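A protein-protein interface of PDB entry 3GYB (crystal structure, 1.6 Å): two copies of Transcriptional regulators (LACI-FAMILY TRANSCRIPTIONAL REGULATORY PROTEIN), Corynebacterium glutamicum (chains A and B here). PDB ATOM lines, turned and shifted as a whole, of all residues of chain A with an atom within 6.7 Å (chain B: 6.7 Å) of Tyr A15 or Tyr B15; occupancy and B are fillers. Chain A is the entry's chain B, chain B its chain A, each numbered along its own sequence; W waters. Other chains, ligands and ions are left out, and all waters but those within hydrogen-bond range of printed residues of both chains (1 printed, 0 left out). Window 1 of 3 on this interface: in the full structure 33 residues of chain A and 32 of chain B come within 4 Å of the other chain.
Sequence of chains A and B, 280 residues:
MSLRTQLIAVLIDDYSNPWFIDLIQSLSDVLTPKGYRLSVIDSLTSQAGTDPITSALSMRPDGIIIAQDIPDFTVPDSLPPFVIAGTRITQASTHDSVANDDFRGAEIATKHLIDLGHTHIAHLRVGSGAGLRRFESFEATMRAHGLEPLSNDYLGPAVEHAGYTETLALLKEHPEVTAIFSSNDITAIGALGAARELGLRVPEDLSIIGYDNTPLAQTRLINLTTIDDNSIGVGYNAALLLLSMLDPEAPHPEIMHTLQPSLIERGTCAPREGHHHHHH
The side-chain hydroxyl of Ser A46 lies within hydrogen-bond range of the backbone carbonyl oxygen of Leu B38 (2.7 Å). OG of Ser A39 is in hydrogen-bond range of OG of Ser B39. The side-chain hydroxyl (OG) of Ser B39 sits at hydrogen-bond distance from the backbone carbonyl oxygen (O) of Val A40 (3.1 Å). The backbone carbonyl oxygen (O) of Val B40 is in hydrogen-bond range of the backbone NH (N) of Val A40, at 2.8 Å.
N of Ile B41 sits at hydrogen-bond distance from O of Val B10. The backbone NH (N) of Ile B12 is in hydrogen-bond range of the backbone carbonyl oxygen (O) of Ile B41 (2.9 Å). The backbone NH (N) of Ser B16 is in hydrogen-bond range of the side-chain carboxylate (OD1) of Asp B14. The side-chain hydroxyl (OG1) of Thr B45 is in hydrogen-bond range of the side-chain carboxylate (OD2) of Asp B42, 2.8 Å away. The side-chain hydroxyl (OG1) of Thr A45 sits at hydrogen-bond distance from the side-chain carboxylate (OD2) of Asp A42 (2.8 Å). N of Ser A46 sits at hydrogen-bond distance from OD1 of Asp A42, at 2.7 Å.
Among the printed residues, pairs that only touch across the chains: Tyr A15 with Tyr B15 (3.6 Å), Tyr A15 with Ile B21 (3.8 Å), Tyr A15 with Val B40 (3.2 Å), Ser A16 with Ile B21 (3.7 Å), Phe A20 with Tyr B15 (3.9 Å), Ile A21 with Tyr B15 (3.8 Å), Ile A21 with Ser B16 (3.7 Å), Ile A24 with Thr B45 (3.6 Å), Ser A39 with Val B40 (3.4 Å), Ser A39 with Ile B41 (3.5 Å), Val A40 with Tyr B15 (3.1 Å), Ile A41 with Ser B39 (3.9 Å), Thr A45 with Ile B24 (3.6 Å) and Thr A45 with Leu B38 (3.7 Å).
Of the printed residues of chain B, Tyr A15 touches Tyr B15, Ile B21 and Val B40. Printed residues of chain B within 4 Å of Ser A39: Ser B39 (3.2 Å), Val B40 (3.4 Å) and Ile B41 (3.5 Å). Tyr B15 touches four residues of chain A. Of the printed residues of chain A, Ser B16 touches Ile A21. Printed residues of chain A within 4 Å of Ile B24: Thr A45. Of the printed residues of chain A, Ser B39 touches Ser A39 (3.2 Å), Val A40 (3.1 Å) and Ile A41 (3.9 Å). The nearest residue of chain A that does not touch Tyr B15 is Ile A24 (4.7 Å).
Of the 18 printed residues of chain A, 10 touch a printed residue of chain B. Hydrophobic or aromatic side chains of chain A that line the printed part of chain B: Tyr A15, Phe A20, Ile A21, Ile A24, Val A40 and Ile A41. Hydrophobic or aromatic side chains of chain B within 4 Å of the printed part of chain A: Tyr B15, Ile B21, Ile B24, Leu B38, Val B40 and Ile B41. Among the printed residues, 18 pairs touch across the chains.
Ser A39 touches its own counterpart, Ser B39. Ser A39 touches Val B40, and with the chains exchanged Val A40 touches Ser B39. Ser A39 touches Ile B41, and with the chains exchanged Ile A41 touches Ser B39. Val B40 touches its own counterpart, Val A40. Positions printed for both chains: 12, 13, 14, 15, 16, 17, 18, 20, 21, 24, 39, 40, 41, 42, 44, 45 and 46. Of the 18 pairs that touch across the chains among the printed residues, 15 have their exchanged pair printed and touching as well.
Water W1 lies within hydrogen-bond range of O of Tyr A15 (3.0 Å) and O of Tyr B15 (3.0 Å).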
ATOM      1  N   ILE A  12      17.416   4.986 -12.166  1.00  0.00           N
ATOM      2  CA  ILE A  12      18.157   5.731 -13.175  1.00  0.00           C
ATOM      3  C   ILE A  12      19.002   4.730 -13.944  1.00  0.00           C
ATOM      4  O   ILE A  12      19.131   3.572 -13.543  1.00  0.00           O
ATOM      5  CB  ILE A  12      19.093   6.787 -12.557  1.00  0.00           C
ATOM      6  CG1 ILE A  12      20.127   6.105 -11.659  1.00  0.00           C
ATOM      7  CG2 ILE A  12      18.276   7.816 -11.793  1.00  0.00           C
ATOM      8  CD1 ILE A  12      21.262   7.010 -11.237  1.00  0.00           C
ATOM      9  N   ASP A  13      19.591   5.169 -15.046  1.00  0.00           N
ATOM     10  CA  ASP A  13      20.388   4.254 -15.839  1.00  0.00           C
ATOM     11  C   ASP A  13      21.862   4.140 -15.483  1.00  0.00           C
ATOM     12  O   ASP A  13      22.356   3.038 -15.229  1.00  0.00           O
ATOM     13  CB  ASP A  13      20.267   4.617 -17.321  1.00  0.00           C
ATOM     14  CG  ASP A  13      18.977   4.116 -17.937  1.00  0.00           C
ATOM     15  OD1 ASP A  13      18.418   4.820 -18.800  1.00  0.00           O
ATOM     16  OD2 ASP A  13      18.529   3.012 -17.561  1.00  0.00           O
ATOM     17  N   ASP A  14      22.547   5.278 -15.428  1.00  0.00           N
ATOM     18  CA  ASP A  14      23.992   5.285 -15.227  1.00  0.00           C
ATOM     19  C   ASP A  14      24.495   6.432 -14.344  1.00  0.00           C
ATOM     20  O   ASP A  14      24.257   7.597 -14.651  1.00  0.00           O
ATOM     21  CB  ASP A  14      24.604   5.394 -16.629  1.00  0.00           C
ATOM     22  CG  ASP A  14      26.099   5.210 -16.655  1.00  0.00           C
ATOM     23  OD1 ASP A  14      26.746   5.230 -15.589  1.00  0.00           O
ATOM     24  OD2 ASP A  14      26.622   5.061 -17.780  1.00  0.00           O
ATOM     25  N   TYR A  15      25.210   6.107 -13.268  1.00  0.00           N
ATOM     26  CA  TYR A  15      25.741   7.138 -12.376  1.00  0.00           C
ATOM     27  C   TYR A  15      26.736   8.033 -13.123  1.00  0.00           C
ATOM     28  O   TYR A  15      27.010   9.155 -12.700  1.00  0.00           O
ATOM     29  CB  TYR A  15      26.445   6.501 -11.167  1.00  0.00           C
ATOM     30  CG  TYR A  15      25.556   5.611 -10.316  1.00  0.00           C
ATOM     31  CD1 TYR A  15      24.407   6.113  -9.711  1.00  0.00           C
ATOM     32  CD2 TYR A  15      25.866   4.266 -10.127  1.00  0.00           C
ATOM     33  CE1 TYR A  15      23.584   5.294  -8.941  1.00  0.00           C
ATOM     34  CE2 TYR A  15      25.049   3.440  -9.359  1.00  0.00           C
ATOM     35  CZ  TYR A  15      23.910   3.958  -8.772  1.00  0.00           C
ATOM     36  OH  TYR A  15      23.078   3.138  -8.042  1.00  0.00           O
ATOM     37  N   SER A  16      27.269   7.525 -14.232  1.00  0.00           N
ATOM     38  CA  SER A  16      28.243   8.253 -15.045  1.00  0.00           C
ATOM     39  C   SER A  16      27.645   9.402 -15.848  1.00  0.00           C
ATOM     40  O   SER A  16      28.370  10.267 -16.345  1.00  0.00           O
ATOM     41  CB  SER A  16      28.964   7.288 -15.992  1.00  0.00           C
ATOM     42  OG  SER A  16      29.764   6.377 -15.255  1.00  0.00           O
ATOM     43  N   ASN A  17      26.325   9.398 -15.980  1.00  0.00           N
ATOM     44  CA  ASN A  17      25.614  10.449 -16.701  1.00  0.00           C
ATOM     45  C   ASN A  17      24.792  11.190 -15.648  1.00  0.00           C
ATOM     46  O   ASN A  17      23.694  10.758 -15.295  1.00  0.00           O
ATOM     47  CB  ASN A  17      24.693   9.839 -17.752  1.00  0.00           C
ATOM     48  CG  ASN A  17      23.893  10.886 -18.487  1.00  0.00           C
ATOM     49  OD1 ASN A  17      24.120  12.082 -18.309  1.00  0.00           O
ATOM     50  ND2 ASN A  17      22.956  10.448 -19.313  1.00  0.00           N
ATOM     51  N   PRO A  18      25.310  12.325 -15.153  1.00  0.00           N
ATOM     52  CA  PRO A  18      24.701  13.178 -14.126  1.00  0.00           C
ATOM     53  C   PRO A  18      23.460  13.985 -14.477  1.00  0.00           C
ATOM     54  O   PRO A  18      23.134  14.950 -13.783  1.00  0.00           O
ATOM     55  CB  PRO A  18      25.855  14.081 -13.718  1.00  0.00           C
ATOM     56  CG  PRO A  18      26.526  14.329 -15.028  1.00  0.00           C
ATOM     57  CD  PRO A  18      26.543  12.948 -15.674  1.00  0.00           C
ATOM     58  N   PHE A  20      20.511  13.226 -14.028  1.00  0.00           N
ATOM     59  CA  PHE A  20      19.534  13.012 -12.962  1.00  0.00           C
ATOM     60  C   PHE A  20      19.775  13.702 -11.627  1.00  0.00           C
ATOM     61  O   PHE A  20      18.872  13.748 -10.787  1.00  0.00           O
ATOM     62  CB  PHE A  20      19.427  11.518 -12.672  1.00  0.00           C
ATOM     63  CG  PHE A  20      20.679  10.943 -12.078  1.00  0.00           C
ATOM     64  CD1 PHE A  20      21.717  10.504 -12.895  1.00  0.00           C
ATOM     65  CD2 PHE A  20      20.851  10.901 -10.696  1.00  0.00           C
ATOM     66  CE1 PHE A  20      22.913  10.034 -12.342  1.00  0.00           C
ATOM     67  CE2 PHE A  20      22.040  10.436 -10.137  1.00  0.00           C
ATOM     68  CZ  PHE A  20      23.073  10.001 -10.965  1.00  0.00           C
ATOM     69  N   ILE A  21      20.974  14.229 -11.414  1.00  0.00           N
ATOM     70  CA  ILE A  21      21.285  14.827 -10.125  1.00  0.00           C
ATOM     71  C   ILE A  21      20.323  15.890  -9.607  1.00  0.00           C
ATOM     72  O   ILE A  21      19.795  15.732  -8.504  1.00  0.00           O
ATOM     73  CB  ILE A  21      22.738  15.346 -10.085  1.00  0.00           C
ATOM     74  CG1 ILE A  21      23.697  14.169 -10.303  1.00  0.00           C
ATOM     75  CG2 ILE A  21      23.032  15.981  -8.729  1.00  0.00           C
ATOM     76  CD1 ILE A  21      25.171  14.534 -10.207  1.00  0.00           C
ATOM     77  N   ILE A  24      16.759  14.424  -8.960  1.00  0.00           N
ATOM     78  CA  ILE A  24      16.577  13.736  -7.684  1.00  0.00           C
ATOM     79  C   ILE A  24      16.548  14.752  -6.545  1.00  0.00           C
ATOM     80  O   ILE A  24      15.818  14.579  -5.570  1.00  0.00           O
ATOM     81  CB  ILE A  24      17.699  12.709  -7.408  1.00  0.00           C
ATOM     82  CG1 ILE A  24      17.601  11.552  -8.404  1.00  0.00           C
ATOM     83  CG2 ILE A  24      17.583  12.180  -5.978  1.00  0.00           C
ATOM     84  CD1 ILE A  24      18.593  10.423  -8.131  1.00  0.00           C
ATOM     85  N   SER A  39      15.841   5.928  -2.259  1.00  0.00           N
ATOM     86  CA  SER A  39      16.970   5.033  -2.488  1.00  0.00           C
ATOM     87  C   SER A  39      17.036   4.858  -3.999  1.00  0.00           C
ATOM     88  O   SER A  39      16.005   4.805  -4.671  1.00  0.00           O
ATOM     89  CB  SER A  39      16.750   3.690  -1.801  1.00  0.00           C
ATOM     90  OG  SER A  39      15.760   2.949  -2.474  1.00  0.00           O
ATOM     91  N   VAL A  40      18.246   4.766  -4.532  1.00  0.00           N
ATOM     92  CA  VAL A  40      18.424   4.650  -5.971  1.00  0.00           C
ATOM     93  C   VAL A  40      18.827   3.275  -6.488  1.00  0.00           C
ATOM     94  O   VAL A  40      19.606   2.560  -5.862  1.00  0.00           O
ATOM     95  CB  VAL A  40      19.467   5.692  -6.450  1.00  0.00           C
ATOM     96  CG1 VAL A  40      19.792   5.497  -7.928  1.00  0.00           C
ATOM     97  CG2 VAL A  40      18.928   7.099  -6.210  1.00  0.00           C
ATOM     98  N   ILE A  41      18.272   2.927  -7.646  1.00  0.00           N
ATOM     99  CA  ILE A  41      18.571   1.673  -8.326  1.00  0.00           C
ATOM    100  C   ILE A  41      18.954   2.038  -9.754  1.00  0.00           C
ATOM    101  O   ILE A  41      18.248   2.806 -10.403  1.00  0.00           O
ATOM    102  CB  ILE A  41      17.344   0.735  -8.338  1.00  0.00           C
ATOM    103  CG1 ILE A  41      17.127   0.188  -6.923  1.00  0.00           C
ATOM    104  CG2 ILE A  41      17.544  -0.399  -9.353  1.00  0.00           C
ATOM    105  CD1 ILE A  41      16.061  -0.856  -6.815  1.00  0.00           C
ATOM    106  N   ASP A  42      20.079   1.514 -10.237  1.00  0.00           N
ATOM    107  CA  ASP A  42      20.507   1.822 -11.596  1.00  0.00           C
ATOM    108  C   ASP A  42      20.274   0.619 -12.502  1.00  0.00           C
ATOM    109  O   ASP A  42      19.648  -0.359 -12.093  1.00  0.00           O
ATOM    110  CB  ASP A  42      21.984   2.264 -11.611  1.00  0.00           C
ATOM    111  CG  ASP A  42      22.958   1.105 -11.526  1.00  0.00           C
ATOM    112  OD1 ASP A  42      22.550   0.001 -11.118  1.00  0.00           O
ATOM    113  OD2 ASP A  42      24.146   1.308 -11.865  1.00  0.00           O
ATOM    114  N   SER A  43      20.753   0.693 -13.735  1.00  0.00           N
ATOM    115  CA  SER A  43      20.558  -0.411 -14.666  1.00  0.00           C
ATOM    116  C   SER A  43      21.856  -1.152 -14.965  1.00  0.00           C
ATOM    117  O   SER A  43      21.859  -2.114 -15.731  1.00  0.00           O
ATOM    118  CB  SER A  43      19.960   0.107 -15.979  1.00  0.00           C
ATOM    119  OG  SER A  43      20.894   0.912 -16.680  1.00  0.00           O
ATOM    120  N   LEU A  44      22.951  -0.721 -14.349  1.00  0.00           N
ATOM    121  CA  LEU A  44      24.241  -1.346 -14.612  1.00  0.00           C
ATOM    122  C   LEU A  44      24.875  -2.097 -13.455  1.00  0.00           C
ATOM    123  O   LEU A  44      25.649  -3.029 -13.677  1.00  0.00           O
ATOM    124  CB  LEU A  44      25.241  -0.290 -15.093  1.00  0.00           C
ATOM    125  CG  LEU A  44      24.893   0.480 -16.366  1.00  0.00           C
ATOM    126  CD1 LEU A  44      25.933   1.569 -16.594  1.00  0.00           C
ATOM    127  CD2 LEU A  44      24.839  -0.473 -17.552  1.00  0.00           C
ATOM    128  N   THR A  45      24.559  -1.708 -12.226  1.00  0.00           N
ATOM    129  CA  THR A  45      25.177  -2.352 -11.077  1.00  0.00           C
ATOM    130  C   THR A  45      24.247  -2.887  -9.994  1.00  0.00           C
ATOM    131  O   THR A  45      24.633  -3.771  -9.230  1.00  0.00           O
ATOM    132  CB  THR A  45      26.189  -1.397 -10.406  1.00  0.00           C
ATOM    133  OG1 THR A  45      25.501  -0.239  -9.913  1.00  0.00           O
ATOM    134  CG2 THR A  45      27.254  -0.955 -11.414  1.00  0.00           C
ATOM    135  N   SER A  46      23.027  -2.369  -9.924  1.00  0.00           N
ATOM    136  CA  SER A  46      22.088  -2.805  -8.895  1.00  0.00           C
ATOM    137  C   SER A  46      21.704  -4.281  -8.958  1.00  0.00           C
ATOM    138  O   SER A  46      21.333  -4.871  -7.941  1.00  0.00           O
ATOM    139  CB  SER A  46      20.825  -1.940  -8.937  1.00  0.00           C
ATOM    140  OG  SER A  46      21.071  -0.675  -8.339  1.00  0.00           O
ATOM    141  N   VAL B  10      24.017   0.659  -0.165  1.00  0.00           N
ATOM    142  CA  VAL B  10      25.319   1.274  -0.348  1.00  0.00           C
ATOM    143  C   VAL B  10      25.182   2.769  -0.081  1.00  0.00           C
ATOM    144  O   VAL B  10      24.432   3.463  -0.770  1.00  0.00           O
ATOM    145  CB  VAL B  10      25.841   1.045  -1.783  1.00  0.00           C
ATOM    146  CG1 VAL B  10      27.234   1.641  -1.931  1.00  0.00           C
ATOM    147  CG2 VAL B  10      25.869  -0.450  -2.089  1.00  0.00           C
ATOM    148  N   ILE B  12      26.670   6.544  -0.023  1.00  0.00           N
ATOM    149  CA  ILE B  12      27.695   7.434  -0.555  1.00  0.00           C
ATOM    150  C   ILE B  12      27.293   8.847  -0.169  1.00  0.00           C
ATOM    151  O   ILE B  12      26.158   9.077   0.247  1.00  0.00           O
ATOM    152  CB  ILE B  12      27.815   7.347  -2.088  1.00  0.00           C
ATOM    153  CG1 ILE B  12      26.491   7.754  -2.734  1.00  0.00           C
ATOM    154  CG2 ILE B  12      28.221   5.933  -2.494  1.00  0.00           C
ATOM    155  CD1 ILE B  12      26.598   7.992  -4.231  1.00  0.00           C
ATOM    156  N   ASP B  13      28.207   9.798  -0.301  1.00  0.00           N
ATOM    157  CA  ASP B  13      27.889  11.165   0.079  1.00  0.00           C
ATOM    158  C   ASP B  13      27.205  12.025  -0.965  1.00  0.00           C
ATOM    159  O   ASP B  13      26.169  12.626  -0.694  1.00  0.00           O
ATOM    160  CB  ASP B  13      29.149  11.915   0.520  1.00  0.00           C
ATOM    161  CG  ASP B  13      29.622  11.504   1.889  1.00  0.00           C
ATOM    162  OD1 ASP B  13      28.788  11.477   2.814  1.00  0.00           O
ATOM    163  OD2 ASP B  13      30.826  11.218   2.036  1.00  0.00           O
ATOM    164  N   ASP B  14      27.780  12.066  -2.160  1.00  0.00           N
ATOM    165  CA  ASP B  14      27.277  12.960  -3.197  1.00  0.00           C
ATOM    166  C   ASP B  14      27.423  12.386  -4.608  1.00  0.00           C
ATOM    167  O   ASP B  14      28.510  11.998  -5.015  1.00  0.00           O
ATOM    168  CB  ASP B  14      28.076  14.259  -3.040  1.00  0.00           C
ATOM    169  CG  ASP B  14      27.652  15.353  -3.985  1.00  0.00           C
ATOM    170  OD1 ASP B  14      26.792  15.121  -4.853  1.00  0.00           O
ATOM    171  OD2 ASP B  14      28.212  16.461  -3.843  1.00  0.00           O
ATOM    172  N   TYR B  15      26.323  12.339  -5.354  1.00  0.00           N
ATOM    173  CA  TYR B  15      26.356  11.820  -6.719  1.00  0.00           C
ATOM    174  C   TYR B  15      27.248  12.670  -7.626  1.00  0.00           C
ATOM    175  O   TYR B  15      27.696  12.202  -8.675  1.00  0.00           O
ATOM    176  CB  TYR B  15      24.936  11.760  -7.298  1.00  0.00           C
ATOM    177  CG  TYR B  15      24.144  10.559  -6.831  1.00  0.00           C
ATOM    178  CD1 TYR B  15      24.494   9.274  -7.246  1.00  0.00           C
ATOM    179  CD2 TYR B  15      23.065  10.701  -5.960  1.00  0.00           C
ATOM    180  CE1 TYR B  15      23.792   8.157  -6.804  1.00  0.00           C
ATOM    181  CE2 TYR B  15      22.353   9.584  -5.507  1.00  0.00           C
ATOM    182  CZ  TYR B  15      22.728   8.318  -5.936  1.00  0.00           C
ATOM    183  OH  TYR B  15      22.048   7.207  -5.497  1.00  0.00           O
ATOM    184  N   SER B  16      27.500  13.912  -7.216  1.00  0.00           N
ATOM    185  CA  SER B  16      28.327  14.839  -7.990  1.00  0.00           C
ATOM    186  C   SER B  16      29.820  14.511  -7.958  1.00  0.00           C
ATOM    187  O   SER B  16      30.593  15.038  -8.763  1.00  0.00           O
ATOM    188  CB  SER B  16      28.111  16.276  -7.498  1.00  0.00           C
ATOM    189  OG  SER B  16      26.778  16.701  -7.731  1.00  0.00           O
ATOM    190  N   ASN B  17      30.223  13.655  -7.022  1.00  0.00           N
ATOM    191  CA  ASN B  17      31.621  13.238  -6.899  1.00  0.00           C
ATOM    192  C   ASN B  17      31.656  11.763  -7.301  1.00  0.00           C
ATOM    193  O   ASN B  17      31.342  10.889  -6.497  1.00  0.00           O
ATOM    194  CB  ASN B  17      32.101  13.416  -5.452  1.00  0.00           C
ATOM    195  CG  ASN B  17      33.547  12.994  -5.261  1.00  0.00           C
ATOM    196  OD1 ASN B  17      34.244  12.678  -6.227  1.00  0.00           O
ATOM    197  ND2 ASN B  17      34.005  12.986  -4.013  1.00  0.00           N
ATOM    198  N   PRO B  18      32.046  11.474  -8.554  1.00  0.00           N
ATOM    199  CA  PRO B  18      32.125  10.125  -9.123  1.00  0.00           C
ATOM    200  C   PRO B  18      33.214   9.182  -8.623  1.00  0.00           C
ATOM    201  O   PRO B  18      33.514   8.194  -9.285  1.00  0.00           O
ATOM    202  CB  PRO B  18      32.257  10.399 -10.618  1.00  0.00           C
ATOM    203  CG  PRO B  18      33.113  11.617 -10.634  1.00  0.00           C
ATOM    204  CD  PRO B  18      32.485  12.476  -9.545  1.00  0.00           C
ATOM    205  N   PHE B  20      33.069   7.049  -6.352  1.00  0.00           N
ATOM    206  CA  PHE B  20      32.443   5.773  -6.004  1.00  0.00           C
ATOM    207  C   PHE B  20      31.971   4.888  -7.155  1.00  0.00           C
ATOM    208  O   PHE B  20      31.669   3.712  -6.947  1.00  0.00           O
ATOM    209  CB  PHE B  20      31.239   6.054  -5.110  1.00  0.00           C
ATOM    210  CG  PHE B  20      30.115   6.746  -5.836  1.00  0.00           C
ATOM    211  CD1 PHE B  20      29.154   6.007  -6.521  1.00  0.00           C
ATOM    212  CD2 PHE B  20      30.065   8.135  -5.903  1.00  0.00           C
ATOM    213  CE1 PHE B  20      28.162   6.641  -7.268  1.00  0.00           C
ATOM    214  CE2 PHE B  20      29.074   8.779  -6.651  1.00  0.00           C
ATOM    215  CZ  PHE B  20      28.124   8.030  -7.333  1.00  0.00           C
ATOM    216  N   ILE B  21      31.898   5.440  -8.359  1.00  0.00           N
ATOM    217  CA  ILE B  21      31.388   4.679  -9.492  1.00  0.00           C
ATOM    218  C   ILE B  21      32.030   3.320  -9.757  1.00  0.00           C
ATOM    219  O   ILE B  21      31.320   2.311  -9.801  1.00  0.00           O
ATOM    220  CB  ILE B  21      31.393   5.536 -10.776  1.00  0.00           C
ATOM    221  CG1 ILE B  21      30.452   6.736 -10.581  1.00  0.00           C
ATOM    222  CG2 ILE B  21      30.924   4.704 -11.966  1.00  0.00           C
ATOM    223  CD1 ILE B  21      30.321   7.638 -11.801  1.00  0.00           C
ATOM    224  N   ILE B  24      31.439   0.835  -6.808  1.00  0.00           N
ATOM    225  CA  ILE B  24      30.146   0.162  -6.802  1.00  0.00           C
ATOM    226  C   ILE B  24      30.116  -0.897  -7.896  1.00  0.00           C
ATOM    227  O   ILE B  24      29.531  -1.965  -7.717  1.00  0.00           O
ATOM    228  CB  ILE B  24      28.981   1.157  -7.012  1.00  0.00           C
ATOM    229  CG1 ILE B  24      28.917   2.129  -5.830  1.00  0.00           C
ATOM    230  CG2 ILE B  24      27.659   0.402  -7.128  1.00  0.00           C
ATOM    231  CD1 ILE B  24      27.702   3.044  -5.858  1.00  0.00           C
ATOM    232  N   LEU B  38      21.693  -4.311  -5.267  1.00  0.00           N
ATOM    233  CA  LEU B  38      22.167  -3.114  -4.577  1.00  0.00           C
ATOM    234  C   LEU B  38      21.293  -1.888  -4.764  1.00  0.00           C
ATOM    235  O   LEU B  38      20.706  -1.693  -5.818  1.00  0.00           O
ATOM    236  CB  LEU B  38      23.569  -2.753  -5.073  1.00  0.00           C
ATOM    237  CG  LEU B  38      24.600  -3.869  -5.239  1.00  0.00           C
ATOM    238  CD1 LEU B  38      25.884  -3.281  -5.808  1.00  0.00           C
ATOM    239  CD2 LEU B  38      24.863  -4.544  -3.906  1.00  0.00           C
ATOM    240  N   SER B  39      21.223  -1.059  -3.725  1.00  0.00           N
ATOM    241  CA  SER B  39      20.469   0.190  -3.789  1.00  0.00           C
ATOM    242  C   SER B  39      21.323   1.238  -3.089  1.00  0.00           C
ATOM    243  O   SER B  39      21.940   0.959  -2.057  1.00  0.00           O
ATOM    244  CB  SER B  39      19.112   0.060  -3.098  1.00  0.00           C
ATOM    245  OG  SER B  39      18.306   1.194  -3.389  1.00  0.00           O
ATOM    246  N   VAL B  40      21.365   2.439  -3.655  1.00  0.00           N
ATOM    247  CA  VAL B  40      22.181   3.513  -3.113  1.00  0.00           C
ATOM    248  C   VAL B  40      21.432   4.567  -2.306  1.00  0.00           C
ATOM    249  O   VAL B  40      20.344   5.009  -2.676  1.00  0.00           O
ATOM    250  CB  VAL B  40      22.959   4.225  -4.251  1.00  0.00           C
ATOM    251  CG1 VAL B  40      23.758   5.394  -3.695  1.00  0.00           C
ATOM    252  CG2 VAL B  40      23.899   3.229  -4.934  1.00  0.00           C
ATOM    253  N   ILE B  41      22.046   4.956  -1.193  1.00  0.00           N
ATOM    254  CA  ILE B  41      21.519   5.977  -0.295  1.00  0.00           C
ATOM    255  C   ILE B  41      22.603   7.055  -0.252  1.00  0.00           C
ATOM    256  O   ILE B  41      23.770   6.740  -0.046  1.00  0.00           O
ATOM    257  CB  ILE B  41      21.325   5.409   1.135  1.00  0.00           C
ATOM    258  CG1 ILE B  41      20.272   4.297   1.129  1.00  0.00           C
ATOM    259  CG2 ILE B  41      20.947   6.531   2.105  1.00  0.00           C
ATOM    260  CD1 ILE B  41      18.859   4.763   0.845  1.00  0.00           C
ATOM    261  N   ASP B  42      22.241   8.319  -0.464  1.00  0.00           N
ATOM    262  CA  ASP B  42      23.248   9.370  -0.421  1.00  0.00           C
ATOM    263  C   ASP B  42      23.064  10.196   0.852  1.00  0.00           C
ATOM    264  O   ASP B  42      22.198   9.889   1.674  1.00  0.00           O
ATOM    265  CB  ASP B  42      23.175  10.244  -1.686  1.00  0.00           C
ATOM    266  CG  ASP B  42      22.102  11.312  -1.613  1.00  0.00           C
ATOM    267  OD1 ASP B  42      21.132  11.145  -0.844  1.00  0.00           O
ATOM    268  OD2 ASP B  42      22.229  12.321  -2.346  1.00  0.00           O
ATOM    269  N   LEU B  44      22.715  13.667   0.769  1.00  0.00           N
ATOM    270  CA  LEU B  44      22.108  14.955   0.452  1.00  0.00           C
ATOM    271  C   LEU B  44      20.652  14.904   0.000  1.00  0.00           C
ATOM    272  O   LEU B  44      19.920  15.883   0.160  1.00  0.00           O
ATOM    273  CB  LEU B  44      22.928  15.659  -0.633  1.00  0.00           C
ATOM    274  CG  LEU B  44      24.401  15.945  -0.343  1.00  0.00           C
ATOM    275  CD1 LEU B  44      25.068  16.504  -1.592  1.00  0.00           C
ATOM    276  CD2 LEU B  44      24.512  16.927   0.810  1.00  0.00           C
ATOM    277  N   THR B  45      20.221  13.775  -0.548  1.00  0.00           N
ATOM    278  CA  THR B  45      18.855  13.685  -1.050  1.00  0.00           C
ATOM    279  C   THR B  45      17.976  12.541  -0.554  1.00  0.00           C
ATOM    280  O   THR B  45      16.752  12.638  -0.616  1.00  0.00           O
ATOM    281  CB  THR B  45      18.852  13.628  -2.587  1.00  0.00           C
ATOM    282  OG1 THR B  45      19.550  12.451  -3.022  1.00  0.00           O
ATOM    283  CG2 THR B  45      19.532  14.865  -3.166  1.00  0.00           C
ATOM    284  N   SER B  46      18.577  11.463  -0.070  1.00  0.00           N
ATOM    285  CA  SER B  46      17.787  10.324   0.389  1.00  0.00           C
ATOM    286  C   SER B  46      16.883  10.601   1.583  1.00  0.00           C
ATOM    287  O   SER B  46      15.906   9.887   1.796  1.00  0.00           O
ATOM    288  CB  SER B  46      18.699   9.137   0.707  1.00  0.00           C
ATOM    289  OG  SER B  46      19.211   8.565  -0.486  1.00  0.00           O
HETATM  290  O   HOH W   1      26.413   9.791  -9.877  1.00  0.00           O
